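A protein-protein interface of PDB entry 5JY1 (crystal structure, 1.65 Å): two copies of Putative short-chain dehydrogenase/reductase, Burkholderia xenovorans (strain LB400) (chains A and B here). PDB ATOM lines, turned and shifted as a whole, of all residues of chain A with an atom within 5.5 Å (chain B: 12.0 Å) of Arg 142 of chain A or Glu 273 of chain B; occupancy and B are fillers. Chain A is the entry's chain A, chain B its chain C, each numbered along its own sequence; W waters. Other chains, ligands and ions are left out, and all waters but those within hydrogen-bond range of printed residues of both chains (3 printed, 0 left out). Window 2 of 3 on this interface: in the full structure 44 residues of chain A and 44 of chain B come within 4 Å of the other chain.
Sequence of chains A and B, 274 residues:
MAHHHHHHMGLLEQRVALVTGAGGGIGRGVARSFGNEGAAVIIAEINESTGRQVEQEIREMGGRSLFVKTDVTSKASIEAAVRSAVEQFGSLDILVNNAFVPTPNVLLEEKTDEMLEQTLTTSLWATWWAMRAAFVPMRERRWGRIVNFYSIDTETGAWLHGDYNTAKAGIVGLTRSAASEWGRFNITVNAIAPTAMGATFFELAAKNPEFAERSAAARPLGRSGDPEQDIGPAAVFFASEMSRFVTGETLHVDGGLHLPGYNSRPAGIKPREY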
ATOM      1  N   PRO A 137      -9.652  -7.195  13.013  1.00  0.00           N
ATOM      2  CA  PRO A 137      -8.850  -7.803  11.938  1.00  0.00           C
ATOM      3  C   PRO A 137      -8.305  -9.184  12.286  1.00  0.00           C
ATOM      4  O   PRO A 137      -8.131 -10.006  11.375  1.00  0.00           O
ATOM      5  CB  PRO A 137      -7.721  -6.787  11.718  1.00  0.00           C
ATOM      6  CG  PRO A 137      -7.620  -6.058  13.019  1.00  0.00           C
ATOM      7  CD  PRO A 137      -9.034  -5.944  13.497  1.00  0.00           C
ATOM      8  N   MET A 138      -8.024  -9.464  13.566  1.00  0.00           N
ATOM      9  CA  MET A 138      -7.515 -10.780  13.945  1.00  0.00           C
ATOM     10  C   MET A 138      -8.568 -11.862  13.739  1.00  0.00           C
ATOM     11  O   MET A 138      -8.268 -12.941  13.213  1.00  0.00           O
ATOM     12  CB  MET A 138      -7.047 -10.776  15.405  1.00  0.00           C
ATOM     13  CG  MET A 138      -5.804  -9.961  15.670  1.00  0.00           C
ATOM     14  SD  MET A 138      -5.441  -9.963  17.435  1.00  0.00           S
ATOM     15  CE  MET A 138      -3.959  -8.962  17.492  1.00  0.00           C
ATOM     16  N   ARG A 139      -9.809 -11.598  14.169  1.00  0.00           N
ATOM     17  CA  ARG A 139     -10.885 -12.558  13.937  1.00  0.00           C
ATOM     18  C   ARG A 139     -11.051 -12.847  12.451  1.00  0.00           C
ATOM     19  O   ARG A 139     -11.191 -14.006  12.046  1.00  0.00           O
ATOM     20  CB  ARG A 139     -12.202 -12.033  14.513  1.00  0.00           C
ATOM     21  CG  ARG A 139     -13.408 -12.880  14.139  1.00  0.00           C
ATOM     22  CD  ARG A 139     -14.707 -12.329  14.729  1.00  0.00           C
ATOM     23  NE  ARG A 139     -14.939 -10.945  14.294  1.00  0.00           N
ATOM     24  CZ  ARG A 139     -15.819 -10.115  14.834  1.00  0.00           C
ATOM     25  NH1 ARG A 139     -16.597 -10.519  15.833  1.00  0.00           N
ATOM     26  NH2 ARG A 139     -15.921  -8.870  14.378  1.00  0.00           N
ATOM     27  N   GLU A 140     -11.055 -11.801  11.623  1.00  0.00           N
ATOM     28  CA  GLU A 140     -11.284 -11.998  10.197  1.00  0.00           C
ATOM     29  C   GLU A 140     -10.231 -12.905   9.580  1.00  0.00           C
ATOM     30  O   GLU A 140     -10.538 -13.724   8.702  1.00  0.00           O
ATOM     31  CB  GLU A 140     -11.300 -10.652   9.483  1.00  0.00           C
ATOM     32  CG  GLU A 140     -11.517 -10.803   7.989  1.00  0.00           C
ATOM     33  CD  GLU A 140     -11.473  -9.491   7.258  1.00  0.00           C
ATOM     34  OE1 GLU A 140     -11.133  -9.513   6.050  1.00  0.00           O
ATOM     35  OE2 GLU A 140     -11.775  -8.456   7.888  1.00  0.00           O
ATOM     36  N   ARG A 141      -8.987 -12.778  10.028  1.00  0.00           N
ATOM     37  CA  ARG A 141      -7.875 -13.532   9.465  1.00  0.00           C
ATOM     38  C   ARG A 141      -7.628 -14.843  10.192  1.00  0.00           C
ATOM     39  O   ARG A 141      -6.762 -15.618   9.763  1.00  0.00           O
ATOM     40  CB  ARG A 141      -6.617 -12.666   9.484  1.00  0.00           C
ATOM     41  CG  ARG A 141      -6.701 -11.516   8.492  1.00  0.00           C
ATOM     42  CD  ARG A 141      -5.732 -10.409   8.810  1.00  0.00           C
ATOM     43  NE  ARG A 141      -5.831  -9.341   7.824  1.00  0.00           N
ATOM     44  CZ  ARG A 141      -6.797  -8.421   7.815  1.00  0.00           C
ATOM     45  NH1 ARG A 141      -7.751  -8.435   8.746  1.00  0.00           N
ATOM     46  NH2 ARG A 141      -6.815  -7.487   6.871  1.00  0.00           N
ATOM     47  N   ARG A 142      -8.379 -15.099  11.270  1.00  0.00           N
ATOM     48  CA  ARG A 142      -8.222 -16.305  12.088  1.00  0.00           C
ATOM     49  C   ARG A 142      -6.771 -16.490  12.530  1.00  0.00           C
ATOM     50  O   ARG A 142      -6.220 -17.592  12.478  1.00  0.00           O
ATOM     51  CB  ARG A 142      -8.735 -17.540  11.342  1.00  0.00           C
ATOM     52  CG  ARG A 142     -10.191 -17.440  10.877  1.00  0.00           C
ATOM     53  CD  ARG A 142     -11.140 -17.370  12.060  1.00  0.00           C
ATOM     54  NE  ARG A 142     -12.508 -17.792  11.741  1.00  0.00           N
ATOM     55  CZ  ARG A 142     -13.561 -16.977  11.666  1.00  0.00           C
ATOM     56  NH1 ARG A 142     -13.421 -15.678  11.868  1.00  0.00           N
ATOM     57  NH2 ARG A 142     -14.760 -17.467  11.393  1.00  0.00           N
ATOM     58  N   TRP A 143      -6.150 -15.398  12.978  1.00  0.00           N
ATOM     59  CA  TRP A 143      -4.776 -15.447  13.484  1.00  0.00           C
ATOM     60  C   TRP A 143      -4.534 -14.200  14.317  1.00  0.00           C
ATOM     61  O   TRP A 143      -4.701 -13.082  13.818  1.00  0.00           O
ATOM     62  CB  TRP A 143      -3.757 -15.534  12.324  1.00  0.00           C
ATOM     63  CG  TRP A 143      -2.386 -16.121  12.710  1.00  0.00           C
ATOM     64  CD1 TRP A 143      -1.942 -17.387  12.462  1.00  0.00           C
ATOM     65  CD2 TRP A 143      -1.299 -15.440  13.374  1.00  0.00           C
ATOM     66  NE1 TRP A 143      -0.660 -17.547  12.948  1.00  0.00           N
ATOM     67  CE2 TRP A 143      -0.240 -16.368  13.502  1.00  0.00           C
ATOM     68  CE3 TRP A 143      -1.122 -14.147  13.875  1.00  0.00           C
ATOM     69  CZ2 TRP A 143       0.976 -16.041  14.113  1.00  0.00           C
ATOM     70  CZ3 TRP A 143       0.080 -13.817  14.478  1.00  0.00           C
ATOM     71  CH2 TRP A 143       1.123 -14.764  14.591  1.00  0.00           C
ATOM     72  N   GLY A 144      -4.110 -14.376  15.565  1.00  0.00           N
ATOM     73  CA  GLY A 144      -3.797 -13.232  16.397  1.00  0.00           C
ATOM     74  C   GLY A 144      -2.906 -13.607  17.556  1.00  0.00           C
ATOM     75  O   GLY A 144      -2.948 -14.735  18.058  1.00  0.00           O
ATOM     76  N   ARG A 184     -10.956 -19.785  19.811  1.00  0.00           N
ATOM     77  CA  ARG A 184     -11.686 -20.385  18.704  1.00  0.00           C
ATOM     78  C   ARG A 184     -11.321 -19.748  17.371  1.00  0.00           C
ATOM     79  O   ARG A 184     -11.568 -20.355  16.319  1.00  0.00           O
ATOM     80  CB  ARG A 184     -13.202 -20.275  18.950  1.00  0.00           C
ATOM     81  CG  ARG A 184     -13.812 -18.876  18.807  1.00  0.00           C
ATOM     82  CD  ARG A 184     -15.294 -18.960  19.162  1.00  0.00           C
ATOM     83  NE  ARG A 184     -16.096 -17.759  18.863  1.00  0.00           N
ATOM     84  CZ  ARG A 184     -16.135 -16.674  19.634  1.00  0.00           C
ATOM     85  NH1 ARG A 184     -15.401 -16.597  20.734  1.00  0.00           N
ATOM     86  NH2 ARG A 184     -16.909 -15.643  19.304  1.00  0.00           N
ATOM     87  N   PHE A 185     -10.753 -18.539  17.391  1.00  0.00           N
ATOM     88  CA  PHE A 185     -10.299 -17.864  16.183  1.00  0.00           C
ATOM     89  C   PHE A 185      -8.787 -17.938  16.003  1.00  0.00           C
ATOM     90  O   PHE A 185      -8.243 -17.171  15.206  1.00  0.00           O
ATOM     91  CB  PHE A 185     -10.716 -16.393  16.198  1.00  0.00           C
ATOM     92  CG  PHE A 185     -12.206 -16.166  16.252  1.00  0.00           C
ATOM     93  CD1 PHE A 185     -13.048 -16.712  15.296  1.00  0.00           C
ATOM     94  CD2 PHE A 185     -12.751 -15.373  17.250  1.00  0.00           C
ATOM     95  CE1 PHE A 185     -14.428 -16.477  15.334  1.00  0.00           C
ATOM     96  CE2 PHE A 185     -14.134 -15.123  17.292  1.00  0.00           C
ATOM     97  CZ  PHE A 185     -14.967 -15.681  16.334  1.00  0.00           C
ATOM     98  N   ASN A 186      -8.097 -18.804  16.755  1.00  0.00           N
ATOM     99  CA  ASN A 186      -6.632 -18.873  16.728  1.00  0.00           C
ATOM    100  C   ASN A 186      -6.013 -17.535  17.138  1.00  0.00           C
ATOM    101  O   ASN A 186      -4.992 -17.106  16.596  1.00  0.00           O
ATOM    102  CB  ASN A 186      -6.109 -19.325  15.358  1.00  0.00           C
ATOM    103  CG  ASN A 186      -4.623 -19.614  15.374  1.00  0.00           C
ATOM    104  OD1 ASN A 186      -4.072 -20.023  16.402  1.00  0.00           O
ATOM    105  ND2 ASN A 186      -3.956 -19.378  14.245  1.00  0.00           N
ATOM    106  N   LEU B 107     -20.617 -12.508  25.020  1.00  0.00           N
ATOM    107  CA  LEU B 107     -19.222 -12.740  24.667  1.00  0.00           C
ATOM    108  C   LEU B 107     -18.426 -11.449  24.842  1.00  0.00           C
ATOM    109  O   LEU B 107     -18.976 -10.346  24.834  1.00  0.00           O
ATOM    110  CB  LEU B 107     -19.124 -13.263  23.229  1.00  0.00           C
ATOM    111  CG  LEU B 107     -19.695 -14.681  23.072  1.00  0.00           C
ATOM    112  CD1 LEU B 107     -19.867 -15.064  21.614  1.00  0.00           C
ATOM    113  CD2 LEU B 107     -18.806 -15.703  23.773  1.00  0.00           C
ATOM    114  N   GLU B 109     -16.386  -9.613  23.121  1.00  0.00           N
ATOM    115  CA  GLU B 109     -16.491  -8.561  22.115  1.00  0.00           C
ATOM    116  C   GLU B 109     -17.866  -7.908  22.095  1.00  0.00           C
ATOM    117  O   GLU B 109     -18.020  -6.847  21.478  1.00  0.00           O
ATOM    118  CB  GLU B 109     -16.142  -9.109  20.717  1.00  0.00           C
ATOM    119  CG  GLU B 109     -17.104 -10.164  20.174  1.00  0.00           C
ATOM    120  CD  GLU B 109     -16.734 -11.595  20.561  1.00  0.00           C
ATOM    121  OE1 GLU B 109     -17.200 -12.540  19.881  1.00  0.00           O
ATOM    122  OE2 GLU B 109     -15.991 -11.777  21.543  1.00  0.00           O
ATOM    123  N   TRP B 159     -16.157 -17.954  30.274  1.00  0.00           N
ATOM    124  CA  TRP B 159     -16.884 -17.337  29.167  1.00  0.00           C
ATOM    125  C   TRP B 159     -18.027 -16.483  29.689  1.00  0.00           C
ATOM    126  O   TRP B 159     -18.684 -16.826  30.679  1.00  0.00           O
ATOM    127  CB  TRP B 159     -17.478 -18.395  28.233  1.00  0.00           C
ATOM    128  CG  TRP B 159     -16.497 -19.227  27.448  1.00  0.00           C
ATOM    129  CD1 TRP B 159     -15.654 -20.189  27.945  1.00  0.00           C
ATOM    130  CD2 TRP B 159     -16.288 -19.200  26.028  1.00  0.00           C
ATOM    131  NE1 TRP B 159     -14.923 -20.751  26.915  1.00  0.00           N
ATOM    132  CE2 TRP B 159     -15.301 -20.165  25.731  1.00  0.00           C
ATOM    133  CE3 TRP B 159     -16.841 -18.455  24.977  1.00  0.00           C
ATOM    134  CZ2 TRP B 159     -14.847 -20.394  24.424  1.00  0.00           C
ATOM    135  CZ3 TRP B 159     -16.389 -18.692  23.674  1.00  0.00           C
ATOM    136  CH2 TRP B 159     -15.406 -19.653  23.416  1.00  0.00           C
ATOM    137  N   ARG B 265     -17.692 -22.805  28.008  1.00  0.00           N
ATOM    138  CA  ARG B 265     -18.026 -22.444  26.635  1.00  0.00           C
ATOM    139  C   ARG B 265     -19.523 -22.635  26.393  1.00  0.00           C
ATOM    140  O   ARG B 265     -20.057 -23.721  26.663  1.00  0.00           O
ATOM    141  CB  ARG B 265     -17.229 -23.284  25.638  1.00  0.00           C
ATOM    142  CG  ARG B 265     -17.574 -22.969  24.189  1.00  0.00           C
ATOM    143  CD  ARG B 265     -16.846 -23.892  23.209  1.00  0.00           C
ATOM    144  NE  ARG B 265     -15.394 -23.798  23.328  1.00  0.00           N
ATOM    145  CZ  ARG B 265     -14.615 -24.765  23.806  1.00  0.00           C
ATOM    146  NH1 ARG B 265     -13.299 -24.585  23.880  1.00  0.00           N
ATOM    147  NH2 ARG B 265     -15.151 -25.911  24.204  1.00  0.00           N
ATOM    148  N   PRO B 266     -20.228 -21.624  25.900  1.00  0.00           N
ATOM    149  CA  PRO B 266     -21.669 -21.773  25.659  1.00  0.00           C
ATOM    150  C   PRO B 266     -21.960 -22.789  24.560  1.00  0.00           C
ATOM    151  O   PRO B 266     -21.150 -23.035  23.668  1.00  0.00           O
ATOM    152  CB  PRO B 266     -22.113 -20.365  25.232  1.00  0.00           C
ATOM    153  CG  PRO B 266     -21.019 -19.449  25.666  1.00  0.00           C
ATOM    154  CD  PRO B 266     -19.747 -20.258  25.636  1.00  0.00           C
ATOM    155  N   ALA B 267     -23.164 -23.359  24.628  1.00  0.00           N
ATOM    156  CA  ALA B 267     -23.541 -24.445  23.722  1.00  0.00           C
ATOM    157  C   ALA B 267     -23.449 -24.034  22.255  1.00  0.00           C
ATOM    158  O   ALA B 267     -23.037 -24.834  21.406  1.00  0.00           O
ATOM    159  CB  ALA B 267     -24.957 -24.926  24.048  1.00  0.00           C
ATOM    160  N   GLY B 268     -23.828 -22.802  21.934  1.00  0.00           N
ATOM    161  CA  GLY B 268     -23.929 -22.384  20.548  1.00  0.00           C
ATOM    162  C   GLY B 268     -22.660 -21.870  19.898  1.00  0.00           C
ATOM    163  O   GLY B 268     -22.723 -21.333  18.785  1.00  0.00           O
ATOM    164  N   ILE B 269     -21.512 -22.016  20.551  1.00  0.00           N
ATOM    165  CA  ILE B 269     -20.244 -21.507  20.048  1.00  0.00           C
ATOM    166  C   ILE B 269     -19.357 -22.705  19.741  1.00  0.00           C
ATOM    167  O   ILE B 269     -19.110 -23.545  20.617  1.00  0.00           O
ATOM    168  CB  ILE B 269     -19.580 -20.555  21.057  1.00  0.00           C
ATOM    169  CG1 ILE B 269     -20.453 -19.305  21.279  1.00  0.00           C
ATOM    170  CG2 ILE B 269     -18.196 -20.166  20.592  1.00  0.00           C
ATOM    171  CD1 ILE B 269     -20.704 -18.469  20.014  1.00  0.00           C
ATOM    172  N   LYS B 270     -18.888 -22.789  18.500  1.00  0.00           N
ATOM    173  CA  LYS B 270     -18.024 -23.898  18.103  1.00  0.00           C
ATOM    174  C   LYS B 270     -16.642 -23.751  18.742  1.00  0.00           C
ATOM    175  O   LYS B 270     -16.142 -22.633  18.904  1.00  0.00           O
ATOM    176  CB  LYS B 270     -17.895 -23.961  16.581  1.00  0.00           C
ATOM    177  N   PRO B 271     -16.008 -24.856  19.144  1.00  0.00           N
ATOM    178  CA  PRO B 271     -14.701 -24.734  19.804  1.00  0.00           C
ATOM    179  C   PRO B 271     -13.584 -24.265  18.883  1.00  0.00           C
ATOM    180  O   PRO B 271     -12.599 -23.695  19.375  1.00  0.00           O
ATOM    181  CB  PRO B 271     -14.427 -26.155  20.320  1.00  0.00           C
ATOM    182  CG  PRO B 271     -15.754 -26.850  20.295  1.00  0.00           C
ATOM    183  CD  PRO B 271     -16.526 -26.233  19.176  1.00  0.00           C
ATOM    184  N   ARG B 272     -13.693 -24.512  17.579  1.00  0.00           N
ATOM    185  CA  ARG B 272     -12.637 -24.181  16.625  1.00  0.00           C
ATOM    186  C   ARG B 272     -13.260 -23.613  15.357  1.00  0.00           C
ATOM    187  O   ARG B 272     -14.062 -24.281  14.695  1.00  0.00           O
ATOM    188  CB  ARG B 272     -11.780 -25.416  16.302  1.00  0.00           C
ATOM    189  CG  ARG B 272     -10.772 -25.202  15.176  1.00  0.00           C
ATOM    190  CD  ARG B 272      -9.897 -26.436  14.983  1.00  0.00           C
ATOM    191  NE  ARG B 272      -8.920 -26.233  13.917  1.00  0.00           N
ATOM    192  CZ  ARG B 272      -7.953 -27.094  13.616  1.00  0.00           C
ATOM    193  NH1 ARG B 272      -7.106 -26.821  12.633  1.00  0.00           N
ATOM    194  NH2 ARG B 272      -7.844 -28.235  14.284  1.00  0.00           N
ATOM    195  N   GLU B 273     -12.886 -22.378  15.016  1.00  0.00           N
ATOM    196  CA  GLU B 273     -13.355 -21.731  13.797  1.00  0.00           C
ATOM    197  C   GLU B 273     -12.209 -21.410  12.845  1.00  0.00           C
ATOM    198  O   GLU B 273     -12.365 -20.570  11.950  1.00  0.00           O
ATOM    199  CB  GLU B 273     -14.139 -20.457  14.132  1.00  0.00           C
ATOM    200  CG  GLU B 273     -15.479 -20.720  14.809  1.00  0.00           C
ATOM    201  CD  GLU B 273     -16.552 -21.206  13.839  1.00  0.00           C
ATOM    202  OE1 GLU B 273     -16.256 -21.364  12.635  1.00  0.00           O
ATOM    203  OE2 GLU B 273     -17.703 -21.424  14.276  1.00  0.00           O
ATOM    204  N   TYR B 274     -11.063 -22.061  13.012  1.00  0.00           N
ATOM    205  CA  TYR B 274      -9.922 -21.823  12.131  1.00  0.00           C
ATOM    206  C   TYR B 274      -9.398 -23.115  11.534  1.00  0.00           C
ATOM    207  O   TYR B 274      -9.681 -24.208  12.027  1.00  0.00           O
ATOM    208  CB  TYR B 274      -8.793 -21.114  12.880  1.00  0.00           C
ATOM    209  CG  TYR B 274      -8.184 -21.922  14.000  1.00  0.00           C
ATOM    210  CD1 TYR B 274      -8.703 -21.856  15.287  1.00  0.00           C
ATOM    211  CD2 TYR B 274      -7.082 -22.743  13.776  1.00  0.00           C
ATOM    212  CE1 TYR B 274      -8.150 -22.586  16.318  1.00  0.00           C
ATOM    213  CE2 TYR B 274      -6.522 -23.478  14.802  1.00  0.00           C
ATOM    214  CZ  TYR B 274      -7.057 -23.389  16.073  1.00  0.00           C
ATOM    215  OH  TYR B 274      -6.513 -24.109  17.101  1.00  0.00           O
ATOM    216  OXT TYR B 274      -8.661 -23.084  10.546  1.00  0.00           O
HETATM  217  O   HOH W   1     -17.189 -12.802  17.190  1.00  0.00           O
HETATM  218  O   HOH W   2     -15.118 -20.181  10.660  1.00  0.00           O
HETATM  219  O   HOH W   3     -15.805 -14.311  22.382  1.00  0.00           O
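The guanidinium group of Arg 142 of chain A lies within hydrogen-bond range of the backbone carbonyl oxygen of Glu 273 of chain B, at 2.8 Å.
O of Arg 184 of chain A lies within hydrogen-bond range of N of Glu 273 of chain B, at 2.7 Å.
OE1 of Glu 109 of chain B lies within salt-bridge range of NH2 of Arg 184 of chain A.
The guanidinium group (NH1) of Arg 142 of chain A sits at hydrogen-bond distance from the backbone carbonyl oxygen (O) of Arg 139 of chain A (2.8 Å).
The guanidinium group (NE) of Arg 272 of chain B is in salt-bridge range of the chain-end carboxylate (O) of Tyr 274 of chain B (2.9 Å).
The backbone NH (N) of Gly 144 of chain A sits at hydrogen-bond distance from the backbone carbonyl oxygen (O) of Asn 186 of chain A, 3.0 Å away.
O of Arg 142 of chain A sits close to ND2 of Asn 186 of chain A, 3.4 Å away.
Among the printed residues, pairs that only touch across the chains: Arg 142 of chain A with Tyr 274 of chain B (3.9 Å), Arg 184 of chain A with Leu 107 of chain B (3.8 Å), Arg 184 of chain A with Trp 159 of chain B (3.7 Å), Arg 184 of chain A with Ile 269 of chain B (3.5 Å), Arg 184 of chain A with Lys 270 of chain B (3.8 Å), Arg 184 of chain A with Pro 271 of chain B (3.5 Å), Arg 184 of chain A with Arg 272 of chain B (3.8 Å), Arg 184 of chain A with Tyr 274 of chain B (3.4 Å), Phe 185 of chain A with Tyr 274 of chain B (3.98 Å) and Asn 186 of chain A with Tyr 274 of chain B (3.4 Å).
Met 138 of chain A touches none of the printed residues of chain B.
Arg 142 of chain A touches two residues of chain B.
No residue of chain B comes within 4 Å of Gly 144 of chain A.
Arg 184 of chain A touches just these residues of chain B: Leu 107 (3.8 Å), Glu 109 (3.2 Å), Trp 159 (3.7 Å), Ile 269 (3.5 Å), Lys 270 (3.8 Å), Pro 271 (3.5 Å), Arg 272 (3.8 Å), Glu 273 (2.7 Å) and Tyr 274 (3.4 Å).
Printed residues of chain A within 4 Å of Leu 107 of chain B: Arg 184.
Of the printed residues of chain A, Lys 270 of chain B touches Arg 184 (3.8 Å).
Of chain A, only Arg 142 (2.8 Å) and Arg 184 (2.7 Å) come within 4 Å of Glu 273 of chain B.
Of the 11 printed residues of chain A, 4 touch a printed residue of chain B.
Of the 13 printed residues of chain B, 9 touch a printed residue of chain A.
Among the printed residues, Asp or Glu carboxylates within 4 Å of a Lys or Arg side-chain nitrogen of the other chain: Arg 184 of chain A with Glu 109 of chain B (3.2 Å).
No position is printed for both chains.
Water W2 bridges OE1 of Glu 273 of chain B and NH2 of Arg 142 of chain A.
Water W3 lies within hydrogen-bond range of OE2 of Glu 109 of chain B (2.7 Å) and NH1 of Arg 184 of chain A (2.8 Å).
Water W1 bridges OE1 of Glu 109 of chain B and NH1 of Arg 139 of chain A.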
